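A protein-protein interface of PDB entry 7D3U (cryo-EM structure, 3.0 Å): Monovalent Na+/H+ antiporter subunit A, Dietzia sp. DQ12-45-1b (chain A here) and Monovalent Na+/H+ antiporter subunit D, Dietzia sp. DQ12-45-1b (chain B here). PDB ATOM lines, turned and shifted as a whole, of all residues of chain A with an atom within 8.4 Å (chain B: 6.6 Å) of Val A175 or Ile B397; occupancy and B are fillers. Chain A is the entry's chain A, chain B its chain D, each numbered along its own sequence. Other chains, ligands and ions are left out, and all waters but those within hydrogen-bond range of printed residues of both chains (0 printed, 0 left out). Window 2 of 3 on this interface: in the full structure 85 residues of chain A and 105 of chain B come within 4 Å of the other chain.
Of the printed residues of chain B, Val A125 touches Leu B393. Val A175 touches one residue of chain B. Printed residues of chain A within 4 Å of Lys B392: Leu A168. Printed residues of chain A within 4 Å of Ile B396: Leu A168 (3.8 Å) and Ala A172 (3.6 Å). Of chain A, only Val A175 (3.8 Å) and Val A176 (3.5 Å) come within 4 Å of Ile B397. The nearest residue of chain A that does not touch Ile B397 is Ala A172 (4.1 Å). The nearest printed residue of chain B that does not touch Val A176 is Asp B401 (4.2 Å).
Of the 12 printed residues of chain B, 5 touch a printed residue of chain A. Hydrophobic or aromatic side chains of chain B within 4 Å of the printed part of chain A: Leu B393, Ile B396, Ile B397 and Leu B400. Hydrophobic or aromatic side chains of chain A within 4 Å of the printed part of chain B: Val A125, Leu A168, Ala A172, Leu A173, Val A175 and Val A176. Along chain A the printed residues that touch a printed residue of chain B span positions 125 to 176.
OD1 of Asp A123 sits at hydrogen-bond distance from N of Val A125.
Among the printed residues, merely in contact across the chains: Val A125 with Leu B393, Leu A168 with Lys B392, Leu A168 with Leu B393, Leu A168 with Ile B396, Ala A172 with Ile B396, Ala A172 with Leu B400, Leu A173 with Leu B400, Val A175 with Ile B397, Val A176 with Ile B397 and Val A176 with Leu B400.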
ATOM      1  N   ALA A  60     -10.841 -19.542  12.000  1.00  0.00           N
ATOM      2  CA  ALA A  60     -10.623 -18.213  12.562  1.00  0.00           C
ATOM      3  C   ALA A  60     -11.865 -17.723  13.295  1.00  0.00           C
ATOM      4  O   ALA A  60     -11.790 -17.294  14.451  1.00  0.00           O
ATOM      5  CB  ALA A  60     -10.225 -17.233  11.460  1.00  0.00           C
ATOM      6  N   LEU A  61     -13.018 -17.785  12.635  1.00  0.00           N
ATOM      7  CA  LEU A  61     -14.286 -17.427  13.255  1.00  0.00           C
ATOM      8  C   LEU A  61     -14.821 -18.507  14.184  1.00  0.00           C
ATOM      9  O   LEU A  61     -15.926 -18.350  14.714  1.00  0.00           O
ATOM     10  CB  LEU A  61     -15.327 -17.121  12.177  1.00  0.00           C
ATOM     11  CG  LEU A  61     -15.340 -15.702  11.617  1.00  0.00           C
ATOM     12  CD1 LEU A  61     -14.064 -15.415  10.857  1.00  0.00           C
ATOM     13  CD2 LEU A  61     -16.546 -15.516  10.718  1.00  0.00           C
ATOM     14  N   GLY A  62     -14.075 -19.587  14.397  1.00  0.00           N
ATOM     15  CA  GLY A  62     -14.588 -20.692  15.178  1.00  0.00           C
ATOM     16  C   GLY A  62     -15.712 -21.444  14.508  1.00  0.00           C
ATOM     17  O   GLY A  62     -16.430 -22.192  15.176  1.00  0.00           O
ATOM     18  N   VAL A  63     -15.883 -21.266  13.203  1.00  0.00           N
ATOM     19  CA  VAL A  63     -16.969 -21.876  12.448  1.00  0.00           C
ATOM     20  C   VAL A  63     -16.424 -23.073  11.688  1.00  0.00           C
ATOM     21  O   VAL A  63     -15.392 -22.973  11.013  1.00  0.00           O
ATOM     22  CB  VAL A  63     -17.610 -20.864  11.483  1.00  0.00           C
ATOM     23  CG1 VAL A  63     -18.617 -21.555  10.586  1.00  0.00           C
ATOM     24  CG2 VAL A  63     -18.260 -19.742  12.260  1.00  0.00           C
ATOM     25  N   ASP A 123     -23.801 -26.534  13.439  1.00  0.00           N
ATOM     26  CA  ASP A 123     -23.231 -25.216  13.652  1.00  0.00           C
ATOM     27  C   ASP A 123     -24.283 -24.162  13.344  1.00  0.00           C
ATOM     28  O   ASP A 123     -25.038 -24.288  12.377  1.00  0.00           O
ATOM     29  CB  ASP A 123     -22.000 -25.012  12.769  1.00  0.00           C
ATOM     30  CG  ASP A 123     -21.316 -23.690  13.026  1.00  0.00           C
ATOM     31  OD1 ASP A 123     -21.788 -22.941  13.904  1.00  0.00           O
ATOM     32  OD2 ASP A 123     -20.305 -23.400  12.354  1.00  0.00           O
ATOM     33  N   VAL A 124     -24.339 -23.124  14.177  1.00  0.00           N
ATOM     34  CA  VAL A 124     -25.367 -22.109  13.988  1.00  0.00           C
ATOM     35  C   VAL A 124     -25.065 -21.257  12.760  1.00  0.00           C
ATOM     36  O   VAL A 124     -25.986 -20.786  12.075  1.00  0.00           O
ATOM     37  CB  VAL A 124     -25.512 -21.261  15.265  1.00  0.00           C
ATOM     38  CG1 VAL A 124     -24.291 -20.382  15.480  1.00  0.00           C
ATOM     39  CG2 VAL A 124     -26.784 -20.436  15.214  1.00  0.00           C
ATOM     40  N   VAL A 125     -23.784 -21.074  12.433  1.00  0.00           N
ATOM     41  CA  VAL A 125     -23.431 -20.254  11.282  1.00  0.00           C
ATOM     42  C   VAL A 125     -23.780 -20.970   9.985  1.00  0.00           C
ATOM     43  O   VAL A 125     -24.323 -20.363   9.056  1.00  0.00           O
ATOM     44  CB  VAL A 125     -21.943 -19.866  11.340  1.00  0.00           C
ATOM     45  CG1 VAL A 125     -21.470 -19.374   9.985  1.00  0.00           C
ATOM     46  CG2 VAL A 125     -21.730 -18.803  12.401  1.00  0.00           C
ATOM     47  N   LEU A 168     -29.339 -14.115  12.119  1.00  0.00           N
ATOM     48  CA  LEU A 168     -27.926 -13.758  12.196  1.00  0.00           C
ATOM     49  C   LEU A 168     -27.605 -13.099  13.529  1.00  0.00           C
ATOM     50  O   LEU A 168     -26.576 -13.397  14.145  1.00  0.00           O
ATOM     51  CB  LEU A 168     -27.551 -12.829  11.042  1.00  0.00           C
ATOM     52  CG  LEU A 168     -26.114 -12.833  10.512  1.00  0.00           C
ATOM     53  CD1 LEU A 168     -26.045 -12.023   9.240  1.00  0.00           C
ATOM     54  CD2 LEU A 168     -25.123 -12.287  11.520  1.00  0.00           C
ATOM     55  N   THR A 169     -28.471 -12.194  13.987  1.00  0.00           N
ATOM     56  CA  THR A 169     -28.229 -11.529  15.261  1.00  0.00           C
ATOM     57  C   THR A 169     -28.303 -12.518  16.416  1.00  0.00           C
ATOM     58  O   THR A 169     -27.484 -12.464  17.339  1.00  0.00           O
ATOM     59  CB  THR A 169     -29.230 -10.394  15.461  1.00  0.00           C
ATOM     60  OG1 THR A 169     -29.128  -9.475  14.368  1.00  0.00           O
ATOM     61  CG2 THR A 169     -28.938  -9.654  16.752  1.00  0.00           C
ATOM     62  N   ALA A 170     -29.268 -13.440  16.374  1.00  0.00           N
ATOM     63  CA  ALA A 170     -29.349 -14.462  17.412  1.00  0.00           C
ATOM     64  C   ALA A 170     -28.112 -15.350  17.408  1.00  0.00           C
ATOM     65  O   ALA A 170     -27.579 -15.692  18.469  1.00  0.00           O
ATOM     66  CB  ALA A 170     -30.612 -15.300  17.230  1.00  0.00           C
ATOM     67  N   ALA A 171     -27.635 -15.725  16.220  1.00  0.00           N
ATOM     68  CA  ALA A 171     -26.437 -16.550  16.122  1.00  0.00           C
ATOM     69  C   ALA A 171     -25.222 -15.825  16.679  1.00  0.00           C
ATOM     70  O   ALA A 171     -24.439 -16.406  17.436  1.00  0.00           O
ATOM     71  CB  ALA A 171     -26.195 -16.953  14.669  1.00  0.00           C
ATOM     72  N   ALA A 172     -25.048 -14.555  16.318  1.00  0.00           N
ATOM     73  CA  ALA A 172     -23.904 -13.800  16.813  1.00  0.00           C
ATOM     74  C   ALA A 172     -23.982 -13.605  18.321  1.00  0.00           C
ATOM     75  O   ALA A 172     -22.960 -13.668  19.013  1.00  0.00           O
ATOM     76  CB  ALA A 172     -23.816 -12.456  16.098  1.00  0.00           C
ATOM     77  N   LEU A 173     -25.186 -13.377  18.852  1.00  0.00           N
ATOM     78  CA  LEU A 173     -25.340 -13.237  20.295  1.00  0.00           C
ATOM     79  C   LEU A 173     -24.991 -14.533  21.011  1.00  0.00           C
ATOM     80  O   LEU A 173     -24.279 -14.521  22.022  1.00  0.00           O
ATOM     81  CB  LEU A 173     -26.767 -12.811  20.628  1.00  0.00           C
ATOM     82  CG  LEU A 173     -27.068 -11.323  20.477  1.00  0.00           C
ATOM     83  CD1 LEU A 173     -28.563 -11.074  20.532  1.00  0.00           C
ATOM     84  CD2 LEU A 173     -26.352 -10.533  21.551  1.00  0.00           C
ATOM     85  N   MET A 174     -25.475 -15.664  20.496  1.00  0.00           N
ATOM     86  CA  MET A 174     -25.168 -16.943  21.122  1.00  0.00           C
ATOM     87  C   MET A 174     -23.696 -17.303  20.971  1.00  0.00           C
ATOM     88  O   MET A 174     -23.152 -18.037  21.802  1.00  0.00           O
ATOM     89  CB  MET A 174     -26.051 -18.038  20.528  1.00  0.00           C
ATOM     90  CG  MET A 174     -27.518 -17.893  20.878  1.00  0.00           C
ATOM     91  SD  MET A 174     -28.533 -19.191  20.155  1.00  0.00           S
ATOM     92  CE  MET A 174     -28.176 -18.966  18.417  1.00  0.00           C
ATOM     93  N   VAL A 175     -23.039 -16.799  19.928  1.00  0.00           N
ATOM     94  CA  VAL A 175     -21.617 -17.077  19.750  1.00  0.00           C
ATOM     95  C   VAL A 175     -20.784 -16.249  20.718  1.00  0.00           C
ATOM     96  O   VAL A 175     -19.844 -16.757  21.340  1.00  0.00           O
ATOM     97  CB  VAL A 175     -21.204 -16.828  18.289  1.00  0.00           C
ATOM     98  CG1 VAL A 175     -19.697 -16.689  18.180  1.00  0.00           C
ATOM     99  CG2 VAL A 175     -21.702 -17.954  17.403  1.00  0.00           C
ATOM    100  N   VAL A 176     -21.110 -14.963  20.866  1.00  0.00           N
ATOM    101  CA  VAL A 176     -20.320 -14.120  21.758  1.00  0.00           C
ATOM    102  C   VAL A 176     -20.615 -14.443  23.216  1.00  0.00           C
ATOM    103  O   VAL A 176     -19.760 -14.236  24.086  1.00  0.00           O
ATOM    104  CB  VAL A 176     -20.552 -12.630  21.456  1.00  0.00           C
ATOM    105  CG1 VAL A 176     -20.203 -12.323  20.014  1.00  0.00           C
ATOM    106  CG2 VAL A 176     -21.984 -12.237  21.759  1.00  0.00           C
ATOM    107  N   ARG A 177     -21.810 -14.949  23.520  1.00  0.00           N
ATOM    108  CA  ARG A 177     -22.129 -15.282  24.903  1.00  0.00           C
ATOM    109  C   ARG A 177     -21.552 -16.638  25.296  1.00  0.00           C
ATOM    110  O   ARG A 177     -20.734 -16.734  26.216  1.00  0.00           O
ATOM    111  CB  ARG A 177     -23.642 -15.262  25.120  1.00  0.00           C
ATOM    112  CG  ARG A 177     -24.047 -15.615  26.537  1.00  0.00           C
ATOM    113  CD  ARG A 177     -24.003 -14.390  27.430  1.00  0.00           C
ATOM    114  NE  ARG A 177     -24.410 -14.691  28.798  1.00  0.00           N
ATOM    115  CZ  ARG A 177     -25.013 -13.824  29.602  1.00  0.00           C
ATOM    116  NH1 ARG A 177     -25.286 -12.599  29.175  1.00  0.00           N
ATOM    117  NH2 ARG A 177     -25.346 -14.181  30.834  1.00  0.00           N
ATOM    118  N   THR A 178     -21.971 -17.698  24.610  1.00  0.00           N
ATOM    119  CA  THR A 178     -21.534 -19.047  24.950  1.00  0.00           C
ATOM    120  C   THR A 178     -20.134 -19.370  24.447  1.00  0.00           C
ATOM    121  O   THR A 178     -19.635 -20.465  24.725  1.00  0.00           O
ATOM    122  CB  THR A 178     -22.521 -20.075  24.396  1.00  0.00           C
ATOM    123  OG1 THR A 178     -22.217 -20.335  23.022  1.00  0.00           O
ATOM    124  CG2 THR A 178     -23.946 -19.561  24.511  1.00  0.00           C
ATOM    125  N   GLY A 179     -19.494 -18.461  23.715  1.00  0.00           N
ATOM    126  CA  GLY A 179     -18.123 -18.646  23.291  1.00  0.00           C
ATOM    127  C   GLY A 179     -17.886 -19.734  22.268  1.00  0.00           C
ATOM    128  O   GLY A 179     -16.734 -19.935  21.866  1.00  0.00           O
ATOM    129  N   THR A 180     -18.922 -20.444  21.830  1.00  0.00           N
ATOM    130  CA  THR A 180     -18.765 -21.532  20.878  1.00  0.00           C
ATOM    131  C   THR A 180     -19.888 -21.481  19.856  1.00  0.00           C
ATOM    132  O   THR A 180     -20.987 -21.001  20.144  1.00  0.00           O
ATOM    133  CB  THR A 180     -18.764 -22.899  21.569  1.00  0.00           C
ATOM    134  OG1 THR A 180     -18.786 -23.935  20.579  1.00  0.00           O
ATOM    135  CG2 THR A 180     -19.984 -23.038  22.466  1.00  0.00           C
ATOM    136  N   THR A 181     -19.603 -21.984  18.658  1.00  0.00           N
ATOM    137  CA  THR A 181     -20.590 -22.057  17.586  1.00  0.00           C
ATOM    138  C   THR A 181     -20.890 -23.531  17.334  1.00  0.00           C
ATOM    139  O   THR A 181     -20.374 -24.143  16.399  1.00  0.00           O
ATOM    140  CB  THR A 181     -20.074 -21.368  16.321  1.00  0.00           C
ATOM    141  OG1 THR A 181     -18.858 -21.998  15.901  1.00  0.00           O
ATOM    142  CG2 THR A 181     -19.787 -19.904  16.594  1.00  0.00           C
ATOM    143  N   VAL A 182     -21.753 -24.097  18.178  1.00  0.00           N
ATOM    144  CA  VAL A 182     -22.244 -25.465  18.045  1.00  0.00           C
ATOM    145  C   VAL A 182     -23.675 -25.478  18.562  1.00  0.00           C
ATOM    146  O   VAL A 182     -23.927 -25.122  19.718  1.00  0.00           O
ATOM    147  CB  VAL A 182     -21.389 -26.492  18.817  1.00  0.00           C
ATOM    148  CG1 VAL A 182     -21.810 -27.899  18.446  1.00  0.00           C
ATOM    149  CG2 VAL A 182     -19.904 -26.319  18.553  1.00  0.00           C
ATOM    150  N   ILE A 186     -24.882 -25.029  22.403  1.00  0.00           N
ATOM    151  CA  ILE A 186     -25.487 -23.755  22.779  1.00  0.00           C
ATOM    152  C   ILE A 186     -26.831 -23.962  23.464  1.00  0.00           C
ATOM    153  O   ILE A 186     -27.160 -23.260  24.422  1.00  0.00           O
ATOM    154  CB  ILE A 186     -25.619 -22.855  21.535  1.00  0.00           C
ATOM    155  CG1 ILE A 186     -24.252 -22.318  21.116  1.00  0.00           C
ATOM    156  CG2 ILE A 186     -26.567 -21.705  21.797  1.00  0.00           C
ATOM    157  CD1 ILE A 186     -24.287 -21.510  19.842  1.00  0.00           C
ATOM    158  N   TRP A 192     -29.328 -20.122  29.378  1.00  0.00           N
ATOM    159  CA  TRP A 192     -30.777 -20.006  29.286  1.00  0.00           C
ATOM    160  C   TRP A 192     -31.463 -20.054  30.643  1.00  0.00           C
ATOM    161  O   TRP A 192     -32.648 -19.717  30.730  1.00  0.00           O
ATOM    162  CB  TRP A 192     -31.327 -21.112  28.388  1.00  0.00           C
ATOM    163  CG  TRP A 192     -30.525 -21.308  27.150  1.00  0.00           C
ATOM    164  CD1 TRP A 192     -29.710 -22.359  26.862  1.00  0.00           C
ATOM    165  CD2 TRP A 192     -30.452 -20.425  26.027  1.00  0.00           C
ATOM    166  NE1 TRP A 192     -29.135 -22.188  25.629  1.00  0.00           N
ATOM    167  CE2 TRP A 192     -29.575 -21.007  25.095  1.00  0.00           C
ATOM    168  CE3 TRP A 192     -31.046 -19.198  25.719  1.00  0.00           C
ATOM    169  CZ2 TRP A 192     -29.277 -20.406  23.879  1.00  0.00           C
ATOM    170  CZ3 TRP A 192     -30.746 -18.604  24.512  1.00  0.00           C
ATOM    171  CH2 TRP A 192     -29.871 -19.208  23.606  1.00  0.00           C
ATOM    172  N   PHE A 198     -31.471 -12.545  28.594  1.00  0.00           N
ATOM    173  CA  PHE A 198     -30.805 -12.959  27.366  1.00  0.00           C
ATOM    174  C   PHE A 198     -31.621 -13.993  26.606  1.00  0.00           C
ATOM    175  O   PHE A 198     -31.761 -13.899  25.380  1.00  0.00           O
ATOM    176  CB  PHE A 198     -29.420 -13.523  27.685  1.00  0.00           C
ATOM    177  CG  PHE A 198     -28.648 -13.958  26.476  1.00  0.00           C
ATOM    178  CD1 PHE A 198     -27.999 -13.030  25.683  1.00  0.00           C
ATOM    179  CD2 PHE A 198     -28.568 -15.295  26.134  1.00  0.00           C
ATOM    180  CE1 PHE A 198     -27.287 -13.428  24.572  1.00  0.00           C
ATOM    181  CE2 PHE A 198     -27.858 -15.698  25.023  1.00  0.00           C
ATOM    182  CZ  PHE A 198     -27.217 -14.763  24.242  1.00  0.00           C
ATOM    183  N   ILE A 202     -33.184 -13.669  22.812  1.00  0.00           N
ATOM    184  CA  ILE A 202     -32.937 -14.695  21.804  1.00  0.00           C
ATOM    185  C   ILE A 202     -34.248 -15.318  21.341  1.00  0.00           C
ATOM    186  O   ILE A 202     -34.424 -15.612  20.153  1.00  0.00           O
ATOM    187  CB  ILE A 202     -31.961 -15.752  22.350  1.00  0.00           C
ATOM    188  CG1 ILE A 202     -30.580 -15.137  22.547  1.00  0.00           C
ATOM    189  CG2 ILE A 202     -31.862 -16.930  21.404  1.00  0.00           C
ATOM    190  CD1 ILE A 202     -30.062 -14.428  21.325  1.00  0.00           C
ATOM    191  N   ILE B 321     -10.350  -8.739  17.330  1.00  0.00           N
ATOM    192  CA  ILE B 321     -11.456  -9.191  16.493  1.00  0.00           C
ATOM    193  C   ILE B 321     -12.014  -8.059  15.644  1.00  0.00           C
ATOM    194  O   ILE B 321     -12.316  -8.254  14.463  1.00  0.00           O
ATOM    195  CB  ILE B 321     -12.546  -9.823  17.376  1.00  0.00           C
ATOM    196  CG1 ILE B 321     -11.921 -10.815  18.355  1.00  0.00           C
ATOM    197  CG2 ILE B 321     -13.588 -10.509  16.516  1.00  0.00           C
ATOM    198  CD1 ILE B 321     -12.885 -11.340  19.388  1.00  0.00           C
ATOM    199  N   LYS B 392     -19.635  -9.393   7.267  1.00  0.00           N
ATOM    200  CA  LYS B 392     -20.663  -8.849   8.145  1.00  0.00           C
ATOM    201  C   LYS B 392     -20.826  -9.693   9.402  1.00  0.00           C
ATOM    202  O   LYS B 392     -21.087  -9.155  10.481  1.00  0.00           O
ATOM    203  CB  LYS B 392     -21.989  -8.735   7.400  1.00  0.00           C
ATOM    204  CG  LYS B 392     -23.020  -7.917   8.144  1.00  0.00           C
ATOM    205  CD  LYS B 392     -24.340  -7.903   7.411  1.00  0.00           C
ATOM    206  CE  LYS B 392     -24.909  -9.297   7.269  1.00  0.00           C
ATOM    207  NZ  LYS B 392     -25.922  -9.375   6.184  1.00  0.00           N
ATOM    208  N   LEU B 393     -20.659 -11.011   9.293  1.00  0.00           N
ATOM    209  CA  LEU B 393     -20.783 -11.867  10.466  1.00  0.00           C
ATOM    210  C   LEU B 393     -19.652 -11.606  11.449  1.00  0.00           C
ATOM    211  O   LEU B 393     -19.886 -11.473  12.656  1.00  0.00           O
ATOM    212  CB  LEU B 393     -20.805 -13.333  10.038  1.00  0.00           C
ATOM    213  CG  LEU B 393     -20.670 -14.376  11.146  1.00  0.00           C
ATOM    214  CD1 LEU B 393     -21.808 -14.247  12.142  1.00  0.00           C
ATOM    215  CD2 LEU B 393     -20.633 -15.769  10.550  1.00  0.00           C
ATOM    216  N   SER B 394     -18.415 -11.526  10.952  1.00  0.00           N
ATOM    217  CA  SER B 394     -17.293 -11.216  11.832  1.00  0.00           C
ATOM    218  C   SER B 394     -17.443  -9.829  12.440  1.00  0.00           C
ATOM    219  O   SER B 394     -17.110  -9.618  13.611  1.00  0.00           O
ATOM    220  CB  SER B 394     -15.979 -11.332  11.065  1.00  0.00           C
ATOM    221  OG  SER B 394     -16.144 -10.946   9.713  1.00  0.00           O
ATOM    222  N   LEU B 395     -17.972  -8.876  11.671  1.00  0.00           N
ATOM    223  CA  LEU B 395     -18.147  -7.526  12.193  1.00  0.00           C
ATOM    224  C   LEU B 395     -19.217  -7.484  13.275  1.00  0.00           C
ATOM    225  O   LEU B 395     -19.051  -6.804  14.291  1.00  0.00           O
ATOM    226  CB  LEU B 395     -18.491  -6.566  11.057  1.00  0.00           C
ATOM    227  CG  LEU B 395     -18.424  -5.083  11.408  1.00  0.00           C
ATOM    228  CD1 LEU B 395     -16.989  -4.667  11.662  1.00  0.00           C
ATOM    229  CD2 LEU B 395     -19.033  -4.250  10.299  1.00  0.00           C
ATOM    230  N   ILE B 396     -20.317  -8.213  13.085  1.00  0.00           N
ATOM    231  CA  ILE B 396     -21.366  -8.246  14.100  1.00  0.00           C
ATOM    232  C   ILE B 396     -20.874  -8.965  15.349  1.00  0.00           C
ATOM    233  O   ILE B 396     -21.193  -8.568  16.476  1.00  0.00           O
ATOM    234  CB  ILE B 396     -22.638  -8.896  13.529  1.00  0.00           C
ATOM    235  CG1 ILE B 396     -23.262  -7.991  12.470  1.00  0.00           C
ATOM    236  CG2 ILE B 396     -23.646  -9.159  14.627  1.00  0.00           C
ATOM    237  CD1 ILE B 396     -24.464  -8.595  11.797  1.00  0.00           C
ATOM    238  N   ILE B 397     -20.080 -10.024  15.174  1.00  0.00           N
ATOM    239  CA  ILE B 397     -19.510 -10.718  16.325  1.00  0.00           C
ATOM    240  C   ILE B 397     -18.584  -9.791  17.098  1.00  0.00           C
ATOM    241  O   ILE B 397     -18.629  -9.731  18.333  1.00  0.00           O
ATOM    242  CB  ILE B 397     -18.788 -11.999  15.869  1.00  0.00           C
ATOM    243  CG1 ILE B 397     -19.799 -13.117  15.621  1.00  0.00           C
ATOM    244  CG2 ILE B 397     -17.765 -12.433  16.900  1.00  0.00           C
ATOM    245  CD1 ILE B 397     -19.172 -14.411  15.168  1.00  0.00           C
ATOM    246  N   ALA B 398     -17.745  -9.034  16.387  1.00  0.00           N
ATOM    247  CA  ALA B 398     -16.840  -8.110  17.059  1.00  0.00           C
ATOM    248  C   ALA B 398     -17.589  -6.958  17.713  1.00  0.00           C
ATOM    249  O   ALA B 398     -17.143  -6.438  18.742  1.00  0.00           O
ATOM    250  CB  ALA B 398     -15.808  -7.573  16.070  1.00  0.00           C
ATOM    251  N   ALA B 399     -18.717  -6.543  17.138  1.00  0.00           N
ATOM    252  CA  ALA B 399     -19.483  -5.445  17.714  1.00  0.00           C
ATOM    253  C   ALA B 399     -20.231  -5.882  18.965  1.00  0.00           C
ATOM    254  O   ALA B 399     -20.313  -5.123  19.937  1.00  0.00           O
ATOM    255  CB  ALA B 399     -20.455  -4.883  16.681  1.00  0.00           C
ATOM    256  N   LEU B 400     -20.789  -7.093  18.958  1.00  0.00           N
ATOM    257  CA  LEU B 400     -21.430  -7.611  20.159  1.00  0.00           C
ATOM    258  C   LEU B 400     -20.417  -7.996  21.225  1.00  0.00           C
ATOM    259  O   LEU B 400     -20.748  -7.970  22.415  1.00  0.00           O
ATOM    260  CB  LEU B 400     -22.306  -8.813  19.816  1.00  0.00           C
ATOM    261  CG  LEU B 400     -23.488  -8.529  18.893  1.00  0.00           C
ATOM    262  CD1 LEU B 400     -24.172  -9.819  18.506  1.00  0.00           C
ATOM    263  CD2 LEU B 400     -24.468  -7.592  19.566  1.00  0.00           C
ATOM    264  N   ASP B 401     -19.194  -8.352  20.828  1.00  0.00           N
ATOM    265  CA  ASP B 401     -18.163  -8.672  21.809  1.00  0.00           C
ATOM    266  C   ASP B 401     -17.725  -7.424  22.565  1.00  0.00           C
ATOM    267  O   ASP B 401     -17.600  -7.443  23.794  1.00  0.00           O
ATOM    268  CB  ASP B 401     -16.973  -9.333  21.118  1.00  0.00           C
ATOM    269  CG  ASP B 401     -16.100 -10.108  22.079  1.00  0.00           C
ATOM    270  OD1 ASP B 401     -16.261  -9.937  23.305  1.00  0.00           O
ATOM    271  OD2 ASP B 401     -15.255 -10.897  21.609  1.00  0.00           O
ATOM    272  N   ALA B 402     -17.491  -6.328  21.845  1.00  0.00           N
ATOM    273  CA  ALA B 402     -17.087  -5.076  22.471  1.00  0.00           C
ATOM    274  C   ALA B 402     -18.215  -4.401  23.237  1.00  0.00           C
ATOM    275  O   ALA B 402     -17.983  -3.344  23.833  1.00  0.00           O
ATOM    276  CB  ALA B 402     -16.535  -4.116  21.417  1.00  0.00           C
